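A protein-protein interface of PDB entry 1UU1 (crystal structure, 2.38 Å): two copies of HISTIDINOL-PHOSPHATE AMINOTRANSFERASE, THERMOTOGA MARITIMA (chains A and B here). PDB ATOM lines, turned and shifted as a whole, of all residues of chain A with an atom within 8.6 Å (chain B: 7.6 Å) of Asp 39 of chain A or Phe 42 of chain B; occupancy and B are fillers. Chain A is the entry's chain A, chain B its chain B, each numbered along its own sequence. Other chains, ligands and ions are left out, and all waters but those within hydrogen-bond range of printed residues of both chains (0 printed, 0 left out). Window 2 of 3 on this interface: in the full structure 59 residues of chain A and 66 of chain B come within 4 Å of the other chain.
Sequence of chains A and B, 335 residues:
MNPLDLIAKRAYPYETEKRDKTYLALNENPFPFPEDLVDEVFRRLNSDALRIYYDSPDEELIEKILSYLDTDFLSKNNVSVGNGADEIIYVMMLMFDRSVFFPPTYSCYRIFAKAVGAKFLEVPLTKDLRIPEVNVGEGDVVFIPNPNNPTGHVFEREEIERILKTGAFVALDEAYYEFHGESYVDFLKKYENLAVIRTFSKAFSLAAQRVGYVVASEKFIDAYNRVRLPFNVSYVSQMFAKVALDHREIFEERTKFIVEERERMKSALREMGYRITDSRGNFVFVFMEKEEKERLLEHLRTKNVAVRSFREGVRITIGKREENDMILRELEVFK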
ATOM      1  N   PHE A  33     -22.039 -23.400  -8.880  1.00  0.00           N
ATOM      2  CA  PHE A  33     -20.616 -23.122  -9.017  1.00  0.00           C
ATOM      3  C   PHE A  33     -20.125 -24.196  -9.985  1.00  0.00           C
ATOM      4  O   PHE A  33     -20.542 -25.349  -9.875  1.00  0.00           O
ATOM      5  CB  PHE A  33     -19.910 -23.257  -7.672  1.00  0.00           C
ATOM      6  CG  PHE A  33     -18.561 -22.618  -7.646  1.00  0.00           C
ATOM      7  CD1 PHE A  33     -18.456 -21.253  -7.761  1.00  0.00           C
ATOM      8  CD2 PHE A  33     -17.389 -23.403  -7.636  1.00  0.00           C
ATOM      9  CE1 PHE A  33     -17.225 -20.644  -7.880  1.00  0.00           C
ATOM     10  CE2 PHE A  33     -16.156 -22.824  -7.759  1.00  0.00           C
ATOM     11  CZ  PHE A  33     -16.074 -21.421  -7.885  1.00  0.00           C
ATOM     12  N   PRO A  34     -19.236 -23.849 -10.920  1.00  0.00           N
ATOM     13  CA  PRO A  34     -18.775 -24.887 -11.857  1.00  0.00           C
ATOM     14  C   PRO A  34     -18.161 -26.146 -11.230  1.00  0.00           C
ATOM     15  O   PRO A  34     -17.286 -26.085 -10.360  1.00  0.00           O
ATOM     16  CB  PRO A  34     -17.811 -24.126 -12.764  1.00  0.00           C
ATOM     17  CG  PRO A  34     -18.392 -22.716 -12.757  1.00  0.00           C
ATOM     18  CD  PRO A  34     -18.664 -22.538 -11.269  1.00  0.00           C
ATOM     19  N   GLU A  35     -18.646 -27.299 -11.679  1.00  0.00           N
ATOM     20  CA  GLU A  35     -18.177 -28.591 -11.168  1.00  0.00           C
ATOM     21  C   GLU A  35     -16.672 -28.751 -11.241  1.00  0.00           C
ATOM     22  O   GLU A  35     -16.054 -29.337 -10.371  1.00  0.00           O
ATOM     23  CB  GLU A  35     -18.821 -29.735 -11.945  1.00  0.00           C
ATOM     24  CG  GLU A  35     -19.189 -30.939 -11.086  1.00  0.00           C
ATOM     25  CD  GLU A  35     -19.416 -32.212 -11.909  1.00  0.00           C
ATOM     26  OE1 GLU A  35     -19.745 -33.274 -11.322  1.00  0.00           O
ATOM     27  OE2 GLU A  35     -19.257 -32.146 -13.149  1.00  0.00           O
ATOM     28  N   ASP A  36     -16.083 -28.239 -12.307  1.00  0.00           N
ATOM     29  CA  ASP A  36     -14.641 -28.339 -12.484  1.00  0.00           C
ATOM     30  C   ASP A  36     -13.861 -27.368 -11.586  1.00  0.00           C
ATOM     31  O   ASP A  36     -12.748 -27.655 -11.165  1.00  0.00           O
ATOM     32  CB  ASP A  36     -14.323 -28.085 -13.945  1.00  0.00           C
ATOM     33  CG  ASP A  36     -15.254 -27.062 -14.549  1.00  0.00           C
ATOM     34  OD1 ASP A  36     -16.406 -27.452 -14.880  1.00  0.00           O
ATOM     35  OD2 ASP A  36     -14.852 -25.878 -14.658  1.00  0.00           O
ATOM     36  N   LEU A  37     -14.423 -26.203 -11.301  1.00  0.00           N
ATOM     37  CA  LEU A  37     -13.708 -25.280 -10.430  1.00  0.00           C
ATOM     38  C   LEU A  37     -13.820 -25.862  -9.023  1.00  0.00           C
ATOM     39  O   LEU A  37     -12.906 -25.764  -8.210  1.00  0.00           O
ATOM     40  CB  LEU A  37     -14.296 -23.870 -10.533  1.00  0.00           C
ATOM     41  CG  LEU A  37     -14.269 -23.351 -11.986  1.00  0.00           C
ATOM     42  CD1 LEU A  37     -14.658 -21.871 -12.047  1.00  0.00           C
ATOM     43  CD2 LEU A  37     -12.867 -23.543 -12.556  1.00  0.00           C
ATOM     44  N   VAL A  38     -14.941 -26.509  -8.750  1.00  0.00           N
ATOM     45  CA  VAL A  38     -15.098 -27.144  -7.460  1.00  0.00           C
ATOM     46  C   VAL A  38     -14.011 -28.202  -7.377  1.00  0.00           C
ATOM     47  O   VAL A  38     -13.388 -28.397  -6.327  1.00  0.00           O
ATOM     48  CB  VAL A  38     -16.452 -27.844  -7.311  1.00  0.00           C
ATOM     49  CG1 VAL A  38     -16.494 -28.621  -5.958  1.00  0.00           C
ATOM     50  CG2 VAL A  38     -17.569 -26.813  -7.358  1.00  0.00           C
ATOM     51  N   ASP A  39     -13.768 -28.881  -8.498  1.00  0.00           N
ATOM     52  CA  ASP A  39     -12.759 -29.917  -8.504  1.00  0.00           C
ATOM     53  C   ASP A  39     -11.407 -29.286  -8.267  1.00  0.00           C
ATOM     54  O   ASP A  39     -10.613 -29.764  -7.459  1.00  0.00           O
ATOM     55  CB  ASP A  39     -12.761 -30.673  -9.829  1.00  0.00           C
ATOM     56  CG  ASP A  39     -11.924 -31.939  -9.759  1.00  0.00           C
ATOM     57  OD1 ASP A  39     -10.679 -31.833  -9.653  1.00  0.00           O
ATOM     58  OD2 ASP A  39     -12.528 -33.037  -9.792  1.00  0.00           O
ATOM     59  N   GLU A  40     -11.142 -28.203  -8.977  1.00  0.00           N
ATOM     60  CA  GLU A  40      -9.872 -27.499  -8.809  1.00  0.00           C
ATOM     61  C   GLU A  40      -9.618 -27.047  -7.362  1.00  0.00           C
ATOM     62  O   GLU A  40      -8.477 -27.123  -6.869  1.00  0.00           O
ATOM     63  CB  GLU A  40      -9.820 -26.279  -9.719  1.00  0.00           C
ATOM     64  CG  GLU A  40      -8.494 -25.541  -9.678  1.00  0.00           C
ATOM     65  CD  GLU A  40      -8.456 -24.433 -10.696  1.00  0.00           C
ATOM     66  OE1 GLU A  40      -9.059 -24.629 -11.770  1.00  0.00           O
ATOM     67  OE2 GLU A  40      -7.829 -23.382 -10.446  1.00  0.00           O
ATOM     68  N   VAL A  41     -10.664 -26.575  -6.687  1.00  0.00           N
ATOM     69  CA  VAL A  41     -10.517 -26.128  -5.304  1.00  0.00           C
ATOM     70  C   VAL A  41     -10.033 -27.254  -4.410  1.00  0.00           C
ATOM     71  O   VAL A  41      -9.070 -27.082  -3.674  1.00  0.00           O
ATOM     72  CB  VAL A  41     -11.843 -25.598  -4.692  1.00  0.00           C
ATOM     73  CG1 VAL A  41     -11.642 -25.383  -3.196  1.00  0.00           C
ATOM     74  CG2 VAL A  41     -12.252 -24.267  -5.351  1.00  0.00           C
ATOM     75  N   PHE A  42     -10.698 -28.408  -4.478  1.00  0.00           N
ATOM     76  CA  PHE A  42     -10.307 -29.534  -3.646  1.00  0.00           C
ATOM     77  C   PHE A  42      -8.984 -30.103  -4.092  1.00  0.00           C
ATOM     78  O   PHE A  42      -8.273 -30.728  -3.321  1.00  0.00           O
ATOM     79  CB  PHE A  42     -11.406 -30.605  -3.631  1.00  0.00           C
ATOM     80  CG  PHE A  42     -12.487 -30.319  -2.623  1.00  0.00           C
ATOM     81  CD1 PHE A  42     -13.441 -29.330  -2.856  1.00  0.00           C
ATOM     82  CD2 PHE A  42     -12.475 -30.953  -1.381  1.00  0.00           C
ATOM     83  CE1 PHE A  42     -14.356 -28.981  -1.852  1.00  0.00           C
ATOM     84  CE2 PHE A  42     -13.386 -30.608  -0.375  1.00  0.00           C
ATOM     85  CZ  PHE A  42     -14.321 -29.623  -0.611  1.00  0.00           C
ATOM     86  N   ARG A  43      -8.649 -29.861  -5.343  1.00  0.00           N
ATOM     87  CA  ARG A  43      -7.389 -30.305  -5.876  1.00  0.00           C
ATOM     88  C   ARG A  43      -6.281 -29.545  -5.149  1.00  0.00           C
ATOM     89  O   ARG A  43      -5.318 -30.125  -4.701  1.00  0.00           O
ATOM     90  CB  ARG A  43      -7.350 -29.997  -7.373  1.00  0.00           C
ATOM     91  CG  ARG A  43      -6.560 -30.985  -8.197  1.00  0.00           C
ATOM     92  CD  ARG A  43      -7.172 -31.140  -9.591  1.00  0.00           C
ATOM     93  NE  ARG A  43      -7.348 -32.547  -9.928  1.00  0.00           N
ATOM     94  CZ  ARG A  43      -8.067 -33.393  -9.203  1.00  0.00           C
ATOM     95  NH1 ARG A  43      -8.681 -32.973  -8.108  1.00  0.00           N
ATOM     96  NH2 ARG A  43      -8.168 -34.660  -9.570  1.00  0.00           N
ATOM     97  N   ARG A  44      -6.432 -28.232  -5.046  1.00  0.00           N
ATOM     98  CA  ARG A  44      -5.454 -27.391  -4.364  1.00  0.00           C
ATOM     99  C   ARG A  44      -5.642 -27.392  -2.840  1.00  0.00           C
ATOM    100  O   ARG A  44      -4.988 -26.655  -2.135  1.00  0.00           O
ATOM    101  CB  ARG A  44      -5.591 -25.963  -4.865  1.00  0.00           C
ATOM    102  CG  ARG A  44      -5.609 -25.839  -6.384  1.00  0.00           C
ATOM    103  CD  ARG A  44      -5.773 -24.388  -6.755  1.00  0.00           C
ATOM    104  NE  ARG A  44      -5.025 -23.572  -5.805  1.00  0.00           N
ATOM    105  CZ  ARG A  44      -4.933 -22.248  -5.857  1.00  0.00           C
ATOM    106  NH1 ARG A  44      -4.230 -21.605  -4.935  1.00  0.00           N
ATOM    107  NH2 ARG A  44      -5.534 -21.574  -6.829  1.00  0.00           N
ATOM    108  N   LEU A  45      -6.559 -28.196  -2.334  1.00  0.00           N
ATOM    109  CA  LEU A  45      -6.800 -28.210  -0.909  1.00  0.00           C
ATOM    110  C   LEU A  45      -5.737 -28.982  -0.161  1.00  0.00           C
ATOM    111  O   LEU A  45      -5.526 -30.166  -0.425  1.00  0.00           O
ATOM    112  CB  LEU A  45      -8.158 -28.824  -0.625  1.00  0.00           C
ATOM    113  CG  LEU A  45      -9.169 -27.873   0.018  1.00  0.00           C
ATOM    114  CD1 LEU A  45      -9.312 -26.589  -0.805  1.00  0.00           C
ATOM    115  CD2 LEU A  45     -10.506 -28.584   0.153  1.00  0.00           C
ATOM    116  N   MET A 239      -9.953 -20.367  -0.921  1.00  0.00           N
ATOM    117  CA  MET A 239      -9.563 -21.141  -2.079  1.00  0.00           C
ATOM    118  C   MET A 239     -10.643 -20.975  -3.146  1.00  0.00           C
ATOM    119  O   MET A 239     -10.353 -20.728  -4.299  1.00  0.00           O
ATOM    120  CB  MET A 239      -9.440 -22.631  -1.727  1.00  0.00           C
ATOM    121  CG  MET A 239      -8.568 -23.378  -2.696  1.00  0.00           C
ATOM    122  SD  MET A 239      -6.945 -22.562  -3.014  1.00  0.00           S
ATOM    123  CE  MET A 239      -6.110 -23.015  -1.373  1.00  0.00           C
ATOM    124  N   PHE A 240     -11.898 -21.110  -2.747  1.00  0.00           N
ATOM    125  CA  PHE A 240     -13.010 -20.950  -3.690  1.00  0.00           C
ATOM    126  C   PHE A 240     -12.963 -19.561  -4.384  1.00  0.00           C
ATOM    127  O   PHE A 240     -13.153 -19.445  -5.599  1.00  0.00           O
ATOM    128  CB  PHE A 240     -14.348 -21.120  -2.948  1.00  0.00           C
ATOM    129  CG  PHE A 240     -14.930 -22.499  -3.042  1.00  0.00           C
ATOM    130  CD1 PHE A 240     -15.416 -22.999  -4.255  1.00  0.00           C
ATOM    131  CD2 PHE A 240     -15.020 -23.290  -1.916  1.00  0.00           C
ATOM    132  CE1 PHE A 240     -15.975 -24.257  -4.320  1.00  0.00           C
ATOM    133  CE2 PHE A 240     -15.580 -24.551  -1.980  1.00  0.00           C
ATOM    134  CZ  PHE A 240     -16.057 -25.035  -3.176  1.00  0.00           C
ATOM    135  N   VAL A 243      -9.900 -19.572  -6.938  1.00  0.00           N
ATOM    136  CA  VAL A 243     -10.080 -20.248  -8.202  1.00  0.00           C
ATOM    137  C   VAL A 243     -11.106 -19.503  -9.039  1.00  0.00           C
ATOM    138  O   VAL A 243     -10.951 -19.408 -10.251  1.00  0.00           O
ATOM    139  CB  VAL A 243     -10.488 -21.734  -8.011  1.00  0.00           C
ATOM    140  CG1 VAL A 243      -9.493 -22.419  -7.050  1.00  0.00           C
ATOM    141  CG2 VAL A 243     -11.901 -21.828  -7.490  1.00  0.00           C
ATOM    142  N   ASP B  36      -9.334 -38.829   3.734  1.00  0.00           N
ATOM    143  CA  ASP B  36     -10.513 -39.491   3.172  1.00  0.00           C
ATOM    144  C   ASP B  36     -11.798 -38.766   3.582  1.00  0.00           C
ATOM    145  O   ASP B  36     -12.836 -38.926   2.943  1.00  0.00           O
ATOM    146  CB  ASP B  36     -10.589 -40.969   3.602  1.00  0.00           C
ATOM    147  CG  ASP B  36     -10.751 -41.135   5.096  1.00  0.00           C
ATOM    148  OD1 ASP B  36      -9.906 -40.613   5.851  1.00  0.00           O
ATOM    149  OD2 ASP B  36     -11.725 -41.782   5.533  1.00  0.00           O
ATOM    150  N   LEU B  37     -11.730 -37.975   4.651  1.00  0.00           N
ATOM    151  CA  LEU B  37     -12.900 -37.227   5.094  1.00  0.00           C
ATOM    152  C   LEU B  37     -13.040 -35.943   4.267  1.00  0.00           C
ATOM    153  O   LEU B  37     -14.140 -35.447   4.069  1.00  0.00           O
ATOM    154  CB  LEU B  37     -12.820 -36.932   6.595  1.00  0.00           C
ATOM    155  CG  LEU B  37     -12.961 -38.173   7.498  1.00  0.00           C
ATOM    156  CD1 LEU B  37     -13.481 -37.765   8.882  1.00  0.00           C
ATOM    157  CD2 LEU B  37     -13.945 -39.163   6.885  1.00  0.00           C
ATOM    158  N   VAL B  38     -11.924 -35.424   3.771  1.00  0.00           N
ATOM    159  CA  VAL B  38     -11.937 -34.238   2.921  1.00  0.00           C
ATOM    160  C   VAL B  38     -12.656 -34.715   1.653  1.00  0.00           C
ATOM    161  O   VAL B  38     -13.545 -34.025   1.127  1.00  0.00           O
ATOM    162  CB  VAL B  38     -10.482 -33.760   2.567  1.00  0.00           C
ATOM    163  CG1 VAL B  38     -10.534 -32.634   1.581  1.00  0.00           C
ATOM    164  CG2 VAL B  38      -9.747 -33.309   3.828  1.00  0.00           C
ATOM    165  N   ASP B  39     -12.278 -35.911   1.183  1.00  0.00           N
ATOM    166  CA  ASP B  39     -12.903 -36.521  -0.002  1.00  0.00           C
ATOM    167  C   ASP B  39     -14.394 -36.798   0.249  1.00  0.00           C
ATOM    168  O   ASP B  39     -15.220 -36.661  -0.646  1.00  0.00           O
ATOM    169  CB  ASP B  39     -12.204 -37.840  -0.364  1.00  0.00           C
ATOM    170  CG  ASP B  39     -10.759 -37.640  -0.750  1.00  0.00           C
ATOM    171  OD1 ASP B  39      -9.989 -38.616  -0.678  1.00  0.00           O
ATOM    172  OD2 ASP B  39     -10.386 -36.506  -1.128  1.00  0.00           O
ATOM    173  N   GLU B  40     -14.730 -37.220   1.458  1.00  0.00           N
ATOM    174  CA  GLU B  40     -16.139 -37.434   1.779  1.00  0.00           C
ATOM    175  C   GLU B  40     -16.838 -36.081   1.576  1.00  0.00           C
ATOM    176  O   GLU B  40     -17.833 -35.992   0.870  1.00  0.00           O
ATOM    177  CB  GLU B  40     -16.306 -37.871   3.231  1.00  0.00           C
ATOM    178  CG  GLU B  40     -17.764 -37.904   3.743  1.00  0.00           C
ATOM    179  CD  GLU B  40     -18.658 -38.925   3.041  1.00  0.00           C
ATOM    180  OE1 GLU B  40     -19.892 -38.911   3.281  1.00  0.00           O
ATOM    181  OE2 GLU B  40     -18.129 -39.746   2.253  1.00  0.00           O
ATOM    182  N   VAL B  41     -16.297 -35.026   2.184  1.00  0.00           N
ATOM    183  CA  VAL B  41     -16.886 -33.708   2.057  1.00  0.00           C
ATOM    184  C   VAL B  41     -17.006 -33.312   0.594  1.00  0.00           C
ATOM    185  O   VAL B  41     -18.063 -32.841   0.181  1.00  0.00           O
ATOM    186  CB  VAL B  41     -16.081 -32.668   2.823  1.00  0.00           C
ATOM    187  CG1 VAL B  41     -16.648 -31.293   2.563  1.00  0.00           C
ATOM    188  CG2 VAL B  41     -16.124 -33.000   4.314  1.00  0.00           C
ATOM    189  N   PHE B  42     -15.937 -33.499  -0.181  1.00  0.00           N
ATOM    190  CA  PHE B  42     -15.963 -33.186  -1.611  1.00  0.00           C
ATOM    191  C   PHE B  42     -17.127 -33.910  -2.276  1.00  0.00           C
ATOM    192  O   PHE B  42     -17.839 -33.319  -3.079  1.00  0.00           O
ATOM    193  CB  PHE B  42     -14.664 -33.623  -2.285  1.00  0.00           C
ATOM    194  CG  PHE B  42     -14.711 -33.618  -3.802  1.00  0.00           C
ATOM    195  CD1 PHE B  42     -14.690 -32.412  -4.520  1.00  0.00           C
ATOM    196  CD2 PHE B  42     -14.734 -34.829  -4.502  1.00  0.00           C
ATOM    197  CE1 PHE B  42     -14.688 -32.399  -5.901  1.00  0.00           C
ATOM    198  CE2 PHE B  42     -14.733 -34.855  -5.891  1.00  0.00           C
ATOM    199  CZ  PHE B  42     -14.709 -33.628  -6.608  1.00  0.00           C
ATOM    200  N   ARG B  43     -17.328 -35.181  -1.932  1.00  0.00           N
ATOM    201  CA  ARG B  43     -18.422 -35.968  -2.521  1.00  0.00           C
ATOM    202  C   ARG B  43     -19.835 -35.628  -2.070  1.00  0.00           C
ATOM    203  O   ARG B  43     -20.776 -35.865  -2.807  1.00  0.00           O
ATOM    204  CB  ARG B  43     -18.194 -37.466  -2.330  1.00  0.00           C
ATOM    205  CG  ARG B  43     -17.274 -38.066  -3.346  1.00  0.00           C
ATOM    206  CD  ARG B  43     -17.117 -39.559  -3.109  1.00  0.00           C
ATOM    207  NE  ARG B  43     -15.845 -39.875  -2.474  1.00  0.00           N
ATOM    208  CZ  ARG B  43     -15.685 -40.147  -1.185  1.00  0.00           C
ATOM    209  NH1 ARG B  43     -16.724 -40.157  -0.365  1.00  0.00           N
ATOM    210  NH2 ARG B  43     -14.468 -40.397  -0.718  1.00  0.00           N
ATOM    211  N   ARG B  44     -20.000 -35.099  -0.867  1.00  0.00           N
ATOM    212  CA  ARG B  44     -21.343 -34.726  -0.400  1.00  0.00           C
ATOM    213  C   ARG B  44     -21.702 -33.297  -0.873  1.00  0.00           C
ATOM    214  O   ARG B  44     -22.835 -32.839  -0.762  1.00  0.00           O
ATOM    215  CB  ARG B  44     -21.407 -34.804   1.134  1.00  0.00           C
ATOM    216  CG  ARG B  44     -21.098 -36.199   1.696  1.00  0.00           C
ATOM    217  CD  ARG B  44     -21.181 -36.280   3.232  1.00  0.00           C
ATOM    218  NE  ARG B  44     -22.416 -35.705   3.758  1.00  0.00           N
ATOM    219  CZ  ARG B  44     -22.845 -35.850   5.012  1.00  0.00           C
ATOM    220  NH1 ARG B  44     -22.142 -36.570   5.891  1.00  0.00           N
ATOM    221  NH2 ARG B  44     -23.970 -35.248   5.392  1.00  0.00           N
ATOM    222  N   LEU B  45     -20.719 -32.613  -1.420  1.00  0.00           N
ATOM    223  CA  LEU B  45     -20.893 -31.249  -1.874  1.00  0.00           C
ATOM    224  C   LEU B  45     -21.788 -31.054  -3.111  1.00  0.00           C
ATOM    225  O   LEU B  45     -21.487 -31.534  -4.191  1.00  0.00           O
ATOM    226  CB  LEU B  45     -19.512 -30.678  -2.120  1.00  0.00           C
ATOM    227  CG  LEU B  45     -19.121 -29.536  -1.184  1.00  0.00           C
ATOM    228  CD1 LEU B  45     -19.603 -28.249  -1.829  1.00  0.00           C
ATOM    229  CD2 LEU B  45     -19.713 -29.698   0.237  1.00  0.00           C
ATOM    230  N   ASN B  46     -22.880 -30.331  -2.938  1.00  0.00           N
ATOM    231  CA  ASN B  46     -23.809 -30.077  -4.014  1.00  0.00           C
ATOM    232  C   ASN B  46     -23.416 -28.750  -4.644  1.00  0.00           C
ATOM    233  O   ASN B  46     -23.733 -27.692  -4.080  1.00  0.00           O
ATOM    234  CB  ASN B  46     -25.244 -29.979  -3.447  1.00  0.00           C
ATOM    235  CG  ASN B  46     -26.294 -29.716  -4.527  1.00  0.00           C
ATOM    236  OD1 ASN B  46     -25.983 -29.221  -5.617  1.00  0.00           O
ATOM    237  ND2 ASN B  46     -27.550 -30.028  -4.212  1.00  0.00           N
ATOM    238  N   SER B  47     -22.759 -28.787  -5.806  1.00  0.00           N
ATOM    239  CA  SER B  47     -22.308 -27.554  -6.436  1.00  0.00           C
ATOM    240  C   SER B  47     -23.420 -26.515  -6.580  1.00  0.00           C
ATOM    241  O   SER B  47     -23.173 -25.327  -6.589  1.00  0.00           O
ATOM    242  CB  SER B  47     -21.662 -27.833  -7.804  1.00  0.00           C
ATOM    243  OG  SER B  47     -22.600 -28.315  -8.742  1.00  0.00           O
ATOM    244  N   TYR B 235     -21.340 -23.190   4.012  1.00  0.00           N
ATOM    245  CA  TYR B 235     -21.933 -24.459   3.702  1.00  0.00           C
ATOM    246  C   TYR B 235     -20.808 -25.516   3.788  1.00  0.00           C
ATOM    247  O   TYR B 235     -20.970 -26.556   4.424  1.00  0.00           O
ATOM    248  CB  TYR B 235     -22.532 -24.376   2.293  1.00  0.00           C
ATOM    249  CG  TYR B 235     -22.822 -25.701   1.629  1.00  0.00           C
ATOM    250  CD1 TYR B 235     -23.826 -26.555   2.101  1.00  0.00           C
ATOM    251  CD2 TYR B 235     -22.116 -26.082   0.500  1.00  0.00           C
ATOM    252  CE1 TYR B 235     -24.120 -27.758   1.453  1.00  0.00           C
ATOM    253  CE2 TYR B 235     -22.393 -27.274  -0.164  1.00  0.00           C
ATOM    254  CZ  TYR B 235     -23.385 -28.106   0.306  1.00  0.00           C
ATOM    255  OH  TYR B 235     -23.631 -29.265  -0.388  1.00  0.00           O
ATOM    256  N   VAL B 236     -19.665 -25.225   3.173  1.00  0.00           N
ATOM    257  CA  VAL B 236     -18.549 -26.160   3.223  1.00  0.00           C
ATOM    258  C   VAL B 236     -17.988 -26.361   4.636  1.00  0.00           C
ATOM    259  O   VAL B 236     -17.622 -27.481   5.002  1.00  0.00           O
ATOM    260  CB  VAL B 236     -17.404 -25.751   2.263  1.00  0.00           C
ATOM    261  CG1 VAL B 236     -16.180 -26.629   2.484  1.00  0.00           C
ATOM    262  CG2 VAL B 236     -17.875 -25.944   0.820  1.00  0.00           C
ATOM    263  N   MET B 239     -20.303 -28.635   6.361  1.00  0.00           N
ATOM    264  CA  MET B 239     -20.147 -29.977   5.818  1.00  0.00           C
ATOM    265  C   MET B 239     -18.960 -30.673   6.500  1.00  0.00           C
ATOM    266  O   MET B 239     -19.032 -31.862   6.828  1.00  0.00           O
ATOM    267  CB  MET B 239     -19.919 -29.911   4.316  1.00  0.00           C
ATOM    268  CG  MET B 239     -20.120 -31.242   3.622  1.00  0.00           C
ATOM    269  SD  MET B 239     -21.790 -31.955   3.931  1.00  0.00           S
ATOM    270  CE  MET B 239     -22.710 -31.202   2.565  1.00  0.00           C
ATOM    271  N   PHE B 240     -17.879 -29.928   6.737  1.00  0.00           N
ATOM    272  CA  PHE B 240     -16.708 -30.486   7.397  1.00  0.00           C
ATOM    273  C   PHE B 240     -17.049 -30.920   8.826  1.00  0.00           C
ATOM    274  O   PHE B 240     -16.652 -31.992   9.263  1.00  0.00           O
ATOM    275  CB  PHE B 240     -15.547 -29.475   7.400  1.00  0.00           C
ATOM    276  CG  PHE B 240     -14.564 -29.676   6.259  1.00  0.00           C
ATOM    277  CD1 PHE B 240     -13.694 -30.772   6.251  1.00  0.00           C
ATOM    278  CD2 PHE B 240     -14.531 -28.796   5.180  1.00  0.00           C
ATOM    279  CE1 PHE B 240     -12.814 -30.983   5.190  1.00  0.00           C
ATOM    280  CE2 PHE B 240     -13.653 -28.997   4.112  1.00  0.00           C
ATOM    281  CZ  PHE B 240     -12.794 -30.087   4.113  1.00  0.00           C
ATOM    282  N   VAL B 243     -19.323 -34.125   8.657  1.00  0.00           N
ATOM    283  CA  VAL B 243     -18.576 -35.311   8.311  1.00  0.00           C
ATOM    284  C   VAL B 243     -17.750 -35.673   9.530  1.00  0.00           C
ATOM    285  O   VAL B 243     -17.729 -36.815   9.957  1.00  0.00           O
ATOM    286  CB  VAL B 243     -17.660 -35.069   7.085  1.00  0.00           C
ATOM    287  CG1 VAL B 243     -16.703 -36.232   6.884  1.00  0.00           C
ATOM    288  CG2 VAL B 243     -18.517 -34.919   5.839  1.00  0.00           C
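Among the printed residues, pairs that only touch across the chains: Asp 39 of chain A with Phe 42 of chain B, Phe 42 of chain A with Val 38 of chain B, Phe 42 of chain A with Phe 42 of chain B and Phe 240 of chain A with Val 236 of chain B.
Asp 39 of chain A touches Phe 42 of chain B, but with the chains exchanged Phe 42 of chain A does not touch Asp 39 of chain B (5.6 Å). Phe 42 of chain A touches Val 38 of chain B, but with the chains exchanged Val 38 of chain A does not touch Phe 42 of chain B (4.2 Å). Phe 42 of chain B touches its own counterpart, Phe 42 of chain A. Positions printed for both chains: 36, 37, 38, 39, 40, 41, 42, 43, 44, 45, 239, 240 and 243. Of the 5 pairs that touch across the chains among the printed residues, 1 has its exchanged pair printed and touching as well.
The guanidinium group (NH1) of Arg 43 of chain A lies within salt-bridge range of the side-chain carboxylate (OD1) of Asp 39 of chain A (2.8 Å).
N of Phe 33 of chain A is in hydrogen-bond range of O of Ser 47 of chain B, 3.2 Å away.
Of the printed residues of chain B, Asp 39 of chain A touches Phe 42. Phe 42 of chain B touches just these residues of chain A: Asp 39 (3.9 Å) and Phe 42 (3.6 Å). No residue of chain A comes within 4 Å of Val 41 of chain B. Printed residues of chain A within 4 Å of Val 236 of chain B: Phe 240 (3.9 Å). Printed residues of chain A within 4 Å of Ser 47 of chain B: Phe 33. Val 243 of chain A touches none of the printed residues of chain B.
Hydrophobic or aromatic side chains of chain A within 4 Å of the printed part of chain B: Phe 42 and Phe 240. Of the 17 printed residues of chain B, 4 touch a printed residue of chain A. Among the printed residues, 5 pairs touch across the chains.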
